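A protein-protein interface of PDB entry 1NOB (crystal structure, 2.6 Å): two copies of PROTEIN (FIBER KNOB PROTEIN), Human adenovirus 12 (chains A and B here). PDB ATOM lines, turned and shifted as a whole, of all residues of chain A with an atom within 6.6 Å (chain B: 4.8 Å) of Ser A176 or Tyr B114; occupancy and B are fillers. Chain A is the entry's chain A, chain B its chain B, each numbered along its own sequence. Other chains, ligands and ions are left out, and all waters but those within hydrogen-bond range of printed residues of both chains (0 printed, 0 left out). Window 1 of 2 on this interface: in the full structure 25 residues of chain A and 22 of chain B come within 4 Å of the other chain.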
ATOM      1  N   PRO A  12      35.525   7.598  -6.372  1.00  0.00           N
ATOM      2  CA  PRO A  12      34.111   7.931  -6.163  1.00  0.00           C
ATOM      3  C   PRO A  12      33.068   7.651  -7.252  1.00  0.00           C
ATOM      4  O   PRO A  12      32.008   7.097  -6.954  1.00  0.00           O
ATOM      5  CB  PRO A  12      34.177   9.413  -5.793  1.00  0.00           C
ATOM      6  CG  PRO A  12      35.329   9.884  -6.624  1.00  0.00           C
ATOM      7  CD  PRO A  12      36.340   8.818  -6.272  1.00  0.00           C
ATOM      8  N   ILE A  42      31.941   1.634   3.145  1.00  0.00           N
ATOM      9  CA  ILE A  42      30.685   2.104   2.577  1.00  0.00           C
ATOM     10  C   ILE A  42      30.448   1.464   1.203  1.00  0.00           C
ATOM     11  O   ILE A  42      31.201   1.683   0.254  1.00  0.00           O
ATOM     12  CB  ILE A  42      30.670   3.632   2.474  1.00  0.00           C
ATOM     13  CG1 ILE A  42      30.823   4.227   3.874  1.00  0.00           C
ATOM     14  CG2 ILE A  42      29.334   4.108   1.896  1.00  0.00           C
ATOM     15  CD1 ILE A  42      30.698   5.716   3.923  1.00  0.00           C
ATOM     16  N   VAL A  43      29.397   0.660   1.102  1.00  0.00           N
ATOM     17  CA  VAL A  43      29.109  -0.038  -0.139  1.00  0.00           C
ATOM     18  C   VAL A  43      27.964   0.603  -0.898  1.00  0.00           C
ATOM     19  O   VAL A  43      27.048   1.174  -0.310  1.00  0.00           O
ATOM     20  CB  VAL A  43      28.794  -1.529   0.134  1.00  0.00           C
ATOM     21  CG1 VAL A  43      27.479  -1.662   0.857  1.00  0.00           C
ATOM     22  CG2 VAL A  43      28.799  -2.308  -1.166  1.00  0.00           C
ATOM     23  N   SER A  44      28.020   0.507  -2.216  1.00  0.00           N
ATOM     24  CA  SER A  44      27.006   1.104  -3.056  1.00  0.00           C
ATOM     25  C   SER A  44      26.987   0.351  -4.375  1.00  0.00           C
ATOM     26  O   SER A  44      28.037   0.145  -4.979  1.00  0.00           O
ATOM     27  CB  SER A  44      27.354   2.583  -3.270  1.00  0.00           C
ATOM     28  OG  SER A  44      26.412   3.258  -4.089  1.00  0.00           O
ATOM     29  N   LEU A  45      25.802  -0.079  -4.808  1.00  0.00           N
ATOM     30  CA  LEU A  45      25.661  -0.799  -6.072  1.00  0.00           C
ATOM     31  C   LEU A  45      24.399  -0.366  -6.834  1.00  0.00           C
ATOM     32  O   LEU A  45      23.329  -0.211  -6.247  1.00  0.00           O
ATOM     33  CB  LEU A  45      25.626  -2.310  -5.822  1.00  0.00           C
ATOM     34  CG  LEU A  45      25.608  -3.246  -7.045  1.00  0.00           C
ATOM     35  CD1 LEU A  45      26.843  -3.023  -7.890  1.00  0.00           C
ATOM     36  CD2 LEU A  45      25.536  -4.708  -6.594  1.00  0.00           C
ATOM     37  N   THR A 130      17.744  -1.945   5.142  1.00  0.00           N
ATOM     38  CA  THR A 130      18.008  -0.767   4.332  1.00  0.00           C
ATOM     39  C   THR A 130      16.913  -0.630   3.255  1.00  0.00           C
ATOM     40  O   THR A 130      15.951  -1.408   3.241  1.00  0.00           O
ATOM     41  CB  THR A 130      19.409  -0.828   3.720  1.00  0.00           C
ATOM     42  OG1 THR A 130      19.710   0.434   3.121  1.00  0.00           O
ATOM     43  CG2 THR A 130      19.509  -1.932   2.674  1.00  0.00           C
ATOM     44  N   THR A 174      20.855   0.630  -4.743  1.00  0.00           N
ATOM     45  CA  THR A 174      20.919   0.634  -3.283  1.00  0.00           C
ATOM     46  C   THR A 174      21.566   1.899  -2.799  1.00  0.00           C
ATOM     47  O   THR A 174      22.354   2.500  -3.509  1.00  0.00           O
ATOM     48  CB  THR A 174      21.806  -0.487  -2.727  1.00  0.00           C
ATOM     49  OG1 THR A 174      23.181  -0.172  -2.989  1.00  0.00           O
ATOM     50  CG2 THR A 174      21.463  -1.818  -3.370  1.00  0.00           C
ATOM     51  N   PRO A 175      21.214   2.343  -1.591  1.00  0.00           N
ATOM     52  CA  PRO A 175      21.819   3.553  -1.050  1.00  0.00           C
ATOM     53  C   PRO A 175      23.247   3.199  -0.614  1.00  0.00           C
ATOM     54  O   PRO A 175      23.645   2.038  -0.702  1.00  0.00           O
ATOM     55  CB  PRO A 175      20.900   3.871   0.131  1.00  0.00           C
ATOM     56  CG  PRO A 175      20.527   2.486   0.608  1.00  0.00           C
ATOM     57  CD  PRO A 175      20.150   1.854  -0.690  1.00  0.00           C
ATOM     58  N   SER A 176      24.029   4.190  -0.192  1.00  0.00           N
ATOM     59  CA  SER A 176      25.380   3.917   0.297  1.00  0.00           C
ATOM     60  C   SER A 176      25.125   3.219   1.624  1.00  0.00           C
ATOM     61  O   SER A 176      24.436   3.761   2.487  1.00  0.00           O
ATOM     62  CB  SER A 176      26.154   5.209   0.559  1.00  0.00           C
ATOM     63  OG  SER A 176      26.503   5.855  -0.640  1.00  0.00           O
ATOM     64  N   CYS A 177      25.660   2.021   1.791  1.00  0.00           N
ATOM     65  CA  CYS A 177      25.433   1.296   3.024  1.00  0.00           C
ATOM     66  C   CYS A 177      26.700   1.174   3.837  1.00  0.00           C
ATOM     67  O   CYS A 177      27.780   0.962   3.293  1.00  0.00           O
ATOM     68  CB  CYS A 177      24.865  -0.086   2.710  1.00  0.00           C
ATOM     69  SG  CYS A 177      23.293  -0.032   1.821  1.00  0.00           S
ATOM     70  N   SER A 178      26.558   1.317   5.149  1.00  0.00           N
ATOM     71  CA  SER A 178      27.692   1.230   6.055  1.00  0.00           C
ATOM     72  C   SER A 178      27.847  -0.176   6.613  1.00  0.00           C
ATOM     73  O   SER A 178      26.882  -0.925   6.733  1.00  0.00           O
ATOM     74  CB  SER A 178      27.511   2.191   7.216  1.00  0.00           C
ATOM     75  OG  SER A 178      26.449   1.750   8.034  1.00  0.00           O
ATOM     76  N   PRO B 109      31.061  15.805   2.008  1.00  0.00           N
ATOM     77  CA  PRO B 109      30.756  14.622   1.197  1.00  0.00           C
ATOM     78  C   PRO B 109      31.263  14.820  -0.222  1.00  0.00           C
ATOM     79  O   PRO B 109      30.981  15.837  -0.856  1.00  0.00           O
ATOM     80  CB  PRO B 109      29.233  14.559   1.250  1.00  0.00           C
ATOM     81  CG  PRO B 109      28.915  15.283   2.563  1.00  0.00           C
ATOM     82  CD  PRO B 109      29.809  16.468   2.389  1.00  0.00           C
ATOM     83  N   ASN B 110      31.996  13.827  -0.708  1.00  0.00           N
ATOM     84  CA  ASN B 110      32.593  13.823  -2.045  1.00  0.00           C
ATOM     85  C   ASN B 110      31.562  14.015  -3.170  1.00  0.00           C
ATOM     86  O   ASN B 110      30.699  13.158  -3.368  1.00  0.00           O
ATOM     87  CB  ASN B 110      33.337  12.501  -2.194  1.00  0.00           C
ATOM     88  CG  ASN B 110      34.154  12.423  -3.444  1.00  0.00           C
ATOM     89  OD1 ASN B 110      33.610  12.399  -4.554  1.00  0.00           O
ATOM     90  ND2 ASN B 110      35.483  12.372  -3.281  1.00  0.00           N
ATOM     91  N   VAL B 111      31.650  15.139  -3.894  1.00  0.00           N
ATOM     92  CA  VAL B 111      30.713  15.449  -4.994  1.00  0.00           C
ATOM     93  C   VAL B 111      30.787  14.511  -6.195  1.00  0.00           C
ATOM     94  O   VAL B 111      29.790  14.301  -6.892  1.00  0.00           O
ATOM     95  CB  VAL B 111      30.874  16.908  -5.542  1.00  0.00           C
ATOM     96  CG1 VAL B 111      30.177  17.908  -4.634  1.00  0.00           C
ATOM     97  CG2 VAL B 111      32.331  17.261  -5.663  1.00  0.00           C
ATOM     98  N   SER B 112      31.966  13.963  -6.453  1.00  0.00           N
ATOM     99  CA  SER B 112      32.143  13.041  -7.560  1.00  0.00           C
ATOM    100  C   SER B 112      31.284  11.824  -7.236  1.00  0.00           C
ATOM    101  O   SER B 112      30.556  11.317  -8.076  1.00  0.00           O
ATOM    102  CB  SER B 112      33.618  12.653  -7.664  1.00  0.00           C
ATOM    103  OG  SER B 112      33.871  11.812  -8.778  1.00  0.00           O
ATOM    104  N   ALA B 113      31.366  11.373  -5.991  1.00  0.00           N
ATOM    105  CA  ALA B 113      30.595  10.221  -5.537  1.00  0.00           C
ATOM    106  C   ALA B 113      29.157  10.619  -5.233  1.00  0.00           C
ATOM    107  O   ALA B 113      28.247   9.798  -5.332  1.00  0.00           O
ATOM    108  CB  ALA B 113      31.240   9.612  -4.293  1.00  0.00           C
ATOM    109  N   TYR B 114      28.966  11.885  -4.863  1.00  0.00           N
ATOM    110  CA  TYR B 114      27.640  12.426  -4.543  1.00  0.00           C
ATOM    111  C   TYR B 114      27.466  13.772  -5.256  1.00  0.00           C
ATOM    112  O   TYR B 114      27.772  14.825  -4.696  1.00  0.00           O
ATOM    113  CB  TYR B 114      27.518  12.649  -3.041  1.00  0.00           C
ATOM    114  CG  TYR B 114      27.991  11.494  -2.207  1.00  0.00           C
ATOM    115  CD1 TYR B 114      27.447  10.231  -2.369  1.00  0.00           C
ATOM    116  CD2 TYR B 114      28.957  11.680  -1.224  1.00  0.00           C
ATOM    117  CE1 TYR B 114      27.838   9.178  -1.575  1.00  0.00           C
ATOM    118  CE2 TYR B 114      29.362  10.636  -0.419  1.00  0.00           C
ATOM    119  CZ  TYR B 114      28.796   9.384  -0.598  1.00  0.00           C
ATOM    120  OH  TYR B 114      29.180   8.340   0.208  1.00  0.00           O
ATOM    121  N   PRO B 115      26.963  13.755  -6.499  1.00  0.00           N
ATOM    122  CA  PRO B 115      26.759  14.968  -7.290  1.00  0.00           C
ATOM    123  C   PRO B 115      25.780  15.951  -6.682  1.00  0.00           C
ATOM    124  O   PRO B 115      24.897  15.557  -5.927  1.00  0.00           O
ATOM    125  CB  PRO B 115      26.272  14.412  -8.622  1.00  0.00           C
ATOM    126  CG  PRO B 115      26.917  13.050  -8.660  1.00  0.00           C
ATOM    127  CD  PRO B 115      26.541  12.589  -7.285  1.00  0.00           C
ATOM    128  N   ARG B 116      25.946  17.227  -7.026  1.00  0.00           N
ATOM    129  CA  ARG B 116      25.084  18.300  -6.536  1.00  0.00           C
ATOM    130  C   ARG B 116      23.681  18.278  -7.151  1.00  0.00           C
ATOM    131  O   ARG B 116      22.730  18.781  -6.546  1.00  0.00           O
ATOM    132  CB  ARG B 116      25.739  19.666  -6.771  1.00  0.00           C
ATOM    133  CG  ARG B 116      27.075  19.845  -6.040  1.00  0.00           C
ATOM    134  CD  ARG B 116      27.505  21.315  -6.004  1.00  0.00           C
ATOM    135  NE  ARG B 116      28.769  21.516  -5.302  1.00  0.00           N
ATOM    136  CZ  ARG B 116      29.960  21.170  -5.785  1.00  0.00           C
ATOM    137  NH1 ARG B 116      30.063  20.602  -6.983  1.00  0.00           N
ATOM    138  NH2 ARG B 116      31.056  21.399  -5.074  1.00  0.00           N
ATOM    139  N   ALA B 122      20.060   7.068  -5.481  1.00  0.00           N
ATOM    140  CA  ALA B 122      20.141   6.204  -4.310  1.00  0.00           C
ATOM    141  C   ALA B 122      21.427   6.348  -3.506  1.00  0.00           C
ATOM    142  O   ALA B 122      21.403   6.412  -2.277  1.00  0.00           O
ATOM    143  CB  ALA B 122      19.956   4.760  -4.736  1.00  0.00           C
ATOM    144  N   LYS B 123      22.544   6.413  -4.217  1.00  0.00           N
ATOM    145  CA  LYS B 123      23.869   6.523  -3.615  1.00  0.00           C
ATOM    146  C   LYS B 123      24.121   7.821  -2.820  1.00  0.00           C
ATOM    147  O   LYS B 123      25.037   7.868  -2.010  1.00  0.00           O
ATOM    148  CB  LYS B 123      24.907   6.366  -4.729  1.00  0.00           C
ATOM    149  CG  LYS B 123      26.354   6.348  -4.312  1.00  0.00           C
ATOM    150  CD  LYS B 123      27.197   6.355  -5.579  1.00  0.00           C
ATOM    151  CE  LYS B 123      28.688   6.328  -5.303  1.00  0.00           C
ATOM    152  NZ  LYS B 123      29.444   6.404  -6.588  1.00  0.00           N
ATOM    153  N   SER B 124      23.334   8.869  -3.056  1.00  0.00           N
ATOM    154  CA  SER B 124      23.521  10.123  -2.318  1.00  0.00           C
ATOM    155  C   SER B 124      22.779  10.040  -0.985  1.00  0.00           C
ATOM    156  O   SER B 124      22.551  11.058  -0.313  1.00  0.00           O
ATOM    157  CB  SER B 124      22.971  11.325  -3.106  1.00  0.00           C
ATOM    158  OG  SER B 124      23.645  11.517  -4.341  1.00  0.00           O
ATOM    159  N   GLN B 125      22.401   8.820  -0.602  1.00  0.00           N
ATOM    160  CA  GLN B 125      21.667   8.615   0.640  1.00  0.00           C
ATOM    161  C   GLN B 125      22.074   7.362   1.378  1.00  0.00           C
ATOM    162  O   GLN B 125      22.536   6.385   0.792  1.00  0.00           O
ATOM    163  CB  GLN B 125      20.173   8.533   0.357  1.00  0.00           C
ATOM    164  CG  GLN B 125      19.594   9.747  -0.327  1.00  0.00           C
ATOM    165  CD  GLN B 125      18.469   9.365  -1.248  1.00  0.00           C
ATOM    166  OE1 GLN B 125      17.498   8.728  -0.839  1.00  0.00           O
ATOM    167  NE2 GLN B 125      18.597   9.738  -2.510  1.00  0.00           N
ATOM    168  N   MET B 126      21.884   7.419   2.688  1.00  0.00           N
ATOM    169  CA  MET B 126      22.170   6.312   3.579  1.00  0.00           C
ATOM    170  C   MET B 126      20.872   6.275   4.377  1.00  0.00           C
ATOM    171  O   MET B 126      20.517   7.249   5.052  1.00  0.00           O
ATOM    172  CB  MET B 126      23.392   6.638   4.444  1.00  0.00           C
ATOM    173  CG  MET B 126      23.686   5.608   5.494  1.00  0.00           C
ATOM    174  SD  MET B 126      25.342   5.758   6.183  1.00  0.00           S
ATOM    175  CE  MET B 126      26.311   5.180   4.828  1.00  0.00           C
ATOM    176  N   PHE B 146      23.430  13.485   0.835  1.00  0.00           N
ATOM    177  CA  PHE B 146      24.596  14.330   0.677  1.00  0.00           C
ATOM    178  C   PHE B 146      24.521  15.210  -0.573  1.00  0.00           C
ATOM    179  O   PHE B 146      24.110  14.760  -1.645  1.00  0.00           O
ATOM    180  CB  PHE B 146      25.848  13.468   0.630  1.00  0.00           C
ATOM    181  CG  PHE B 146      25.755  12.232   1.474  1.00  0.00           C
ATOM    182  CD1 PHE B 146      26.140  12.251   2.822  1.00  0.00           C
ATOM    183  CD2 PHE B 146      25.242  11.051   0.942  1.00  0.00           C
ATOM    184  CE1 PHE B 146      26.017  11.117   3.622  1.00  0.00           C
ATOM    185  CE2 PHE B 146      25.113   9.911   1.734  1.00  0.00           C
ATOM    186  CZ  PHE B 146      25.505   9.947   3.081  1.00  0.00           C
ATOM    187  N   ASN B 147      24.912  16.475  -0.414  1.00  0.00           N
ATOM    188  CA  ASN B 147      24.923  17.419  -1.510  1.00  0.00           C
ATOM    189  C   ASN B 147      23.578  17.426  -2.217  1.00  0.00           C
ATOM    190  O   ASN B 147      23.500  17.604  -3.435  1.00  0.00           O
ATOM    191  CB  ASN B 147      26.037  17.044  -2.493  1.00  0.00           C
ATOM    192  CG  ASN B 147      27.389  16.960  -1.826  1.00  0.00           C
ATOM    193  OD1 ASN B 147      27.783  17.851  -1.091  1.00  0.00           O
ATOM    194  ND2 ASN B 147      28.112  15.891  -2.094  1.00  0.00           N
ATOM    195  N   TYR B 181      30.139   8.597   5.538  1.00  0.00           N
ATOM    196  CA  TYR B 181      30.247   8.959   4.119  1.00  0.00           C
ATOM    197  C   TYR B 181      31.664   9.237   3.625  1.00  0.00           C
ATOM    198  O   TYR B 181      32.536   9.608   4.403  1.00  0.00           O
ATOM    199  CB  TYR B 181      29.366  10.178   3.828  1.00  0.00           C
ATOM    200  CG  TYR B 181      29.668  11.408   4.666  1.00  0.00           C
ATOM    201  CD1 TYR B 181      30.797  12.196   4.420  1.00  0.00           C
ATOM    202  CD2 TYR B 181      28.801  11.801   5.690  1.00  0.00           C
ATOM    203  CE1 TYR B 181      31.051  13.357   5.176  1.00  0.00           C
ATOM    204  CE2 TYR B 181      29.038  12.948   6.452  1.00  0.00           C
ATOM    205  CZ  TYR B 181      30.161  13.725   6.195  1.00  0.00           C
ATOM    206  OH  TYR B 181      30.390  14.856   6.959  1.00  0.00           O
ATOM    207  N   ILE B 182      31.870   9.061   2.323  1.00  0.00           N
ATOM    208  CA  ILE B 182      33.164   9.285   1.665  1.00  0.00           C
ATOM    209  C   ILE B 182      33.425  10.788   1.600  1.00  0.00           C
ATOM    210  O   ILE B 182      32.560  11.563   1.171  1.00  0.00           O
ATOM    211  CB  ILE B 182      33.141   8.712   0.229  1.00  0.00           C
ATOM    212  CG1 ILE B 182      32.806   7.217   0.282  1.00  0.00           C
ATOM    213  CG2 ILE B 182      34.456   9.006  -0.480  1.00  0.00           C
ATOM    214  CD1 ILE B 182      32.638   6.555  -1.064  1.00  0.00           C
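Of the 17 printed residues of chain B, 10 touch a printed residue of chain A.
Of the 11 printed residues of chain A, 7 touch a printed residue of chain B.
Hydrophobic or aromatic side chains of chain A within 4 Å of the printed part of chain B: Pro A12, Ile A42 and Pro A175.
Of the printed residues of chain A, Tyr B114 touches Ser A176 (3.7 Å).
Printed residues of chain A within 4 Å of Ala B122: Thr A174 and Pro A175.
Printed residues of chain A within 4 Å of Gln B125: Pro A175 and Ser A176.
Of the printed residues of chain A, Ile B182 touches Ile A42.
Of the printed residues of chain B, Ser A44 touches Lys B123 (3.1 Å).
Pro B109 touches none of the printed residues of chain A.
Ser B124 touches none of the printed residues of chain A.
The nearest residue of chain B that does not touch Ser A176 is Ala B122 (4.02 Å).
The nearest printed residue of chain B that does not touch Ser A44 is Ala B122 (5.9 Å).
No position is printed for both chains.
Of the 16 pairs that touch across the chains among the printed residues, none has its exchanged pair printed and touching as well.
O of Pro A175 is in hydrogen-bond range of SG of Cys A177.
The backbone NH (N) of Ser B112 is in hydrogen-bond range of the side-chain amide oxygen (OD1) of Asn B110.
OD1 of Asn B110 lies within hydrogen-bond range of N of Ala B113.
O of Ile B182 lies within hydrogen-bond range of N of Asn B110, 3.0 Å away.
ND2 of Asn B147 is in hydrogen-bond range of O of Tyr B114 (2.8 Å).
The side-chain hydroxyl (OH) of Tyr B114 lies within hydrogen-bond range of the backbone NH (N) of Ile B182, 3.5 Å away.
NZ of Lys B123 lies within hydrogen-bond range of O of Pro A12, 2.7 Å away.
The side-chain hydroxyl of Ser A176 lies within hydrogen-bond range of the backbone carbonyl oxygen of Lys B123.
N of Ser A176 is in hydrogen-bond range of O of Gln B125, 2.8 Å away.
Ser B112 touches Pro A12.
Ala B113 touches Pro A12.
Ile A42 touches Tyr B181.
Ser A44 touches Lys B123 (OG to CG, 3.1 Å).
Ala B122 touches Thr A174.
N of Lys B123 touches O of Thr A174, 3.98 Å away.
O of Ala B122 touches CA of Pro A175, 3.1 Å away.
Gln B125 touches Pro A175.
Tyr B114 touches Ser A176 (CE1 to OG, 3.7 Å).
CE of Met B126 touches O of Ser A176 (3.3 Å).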
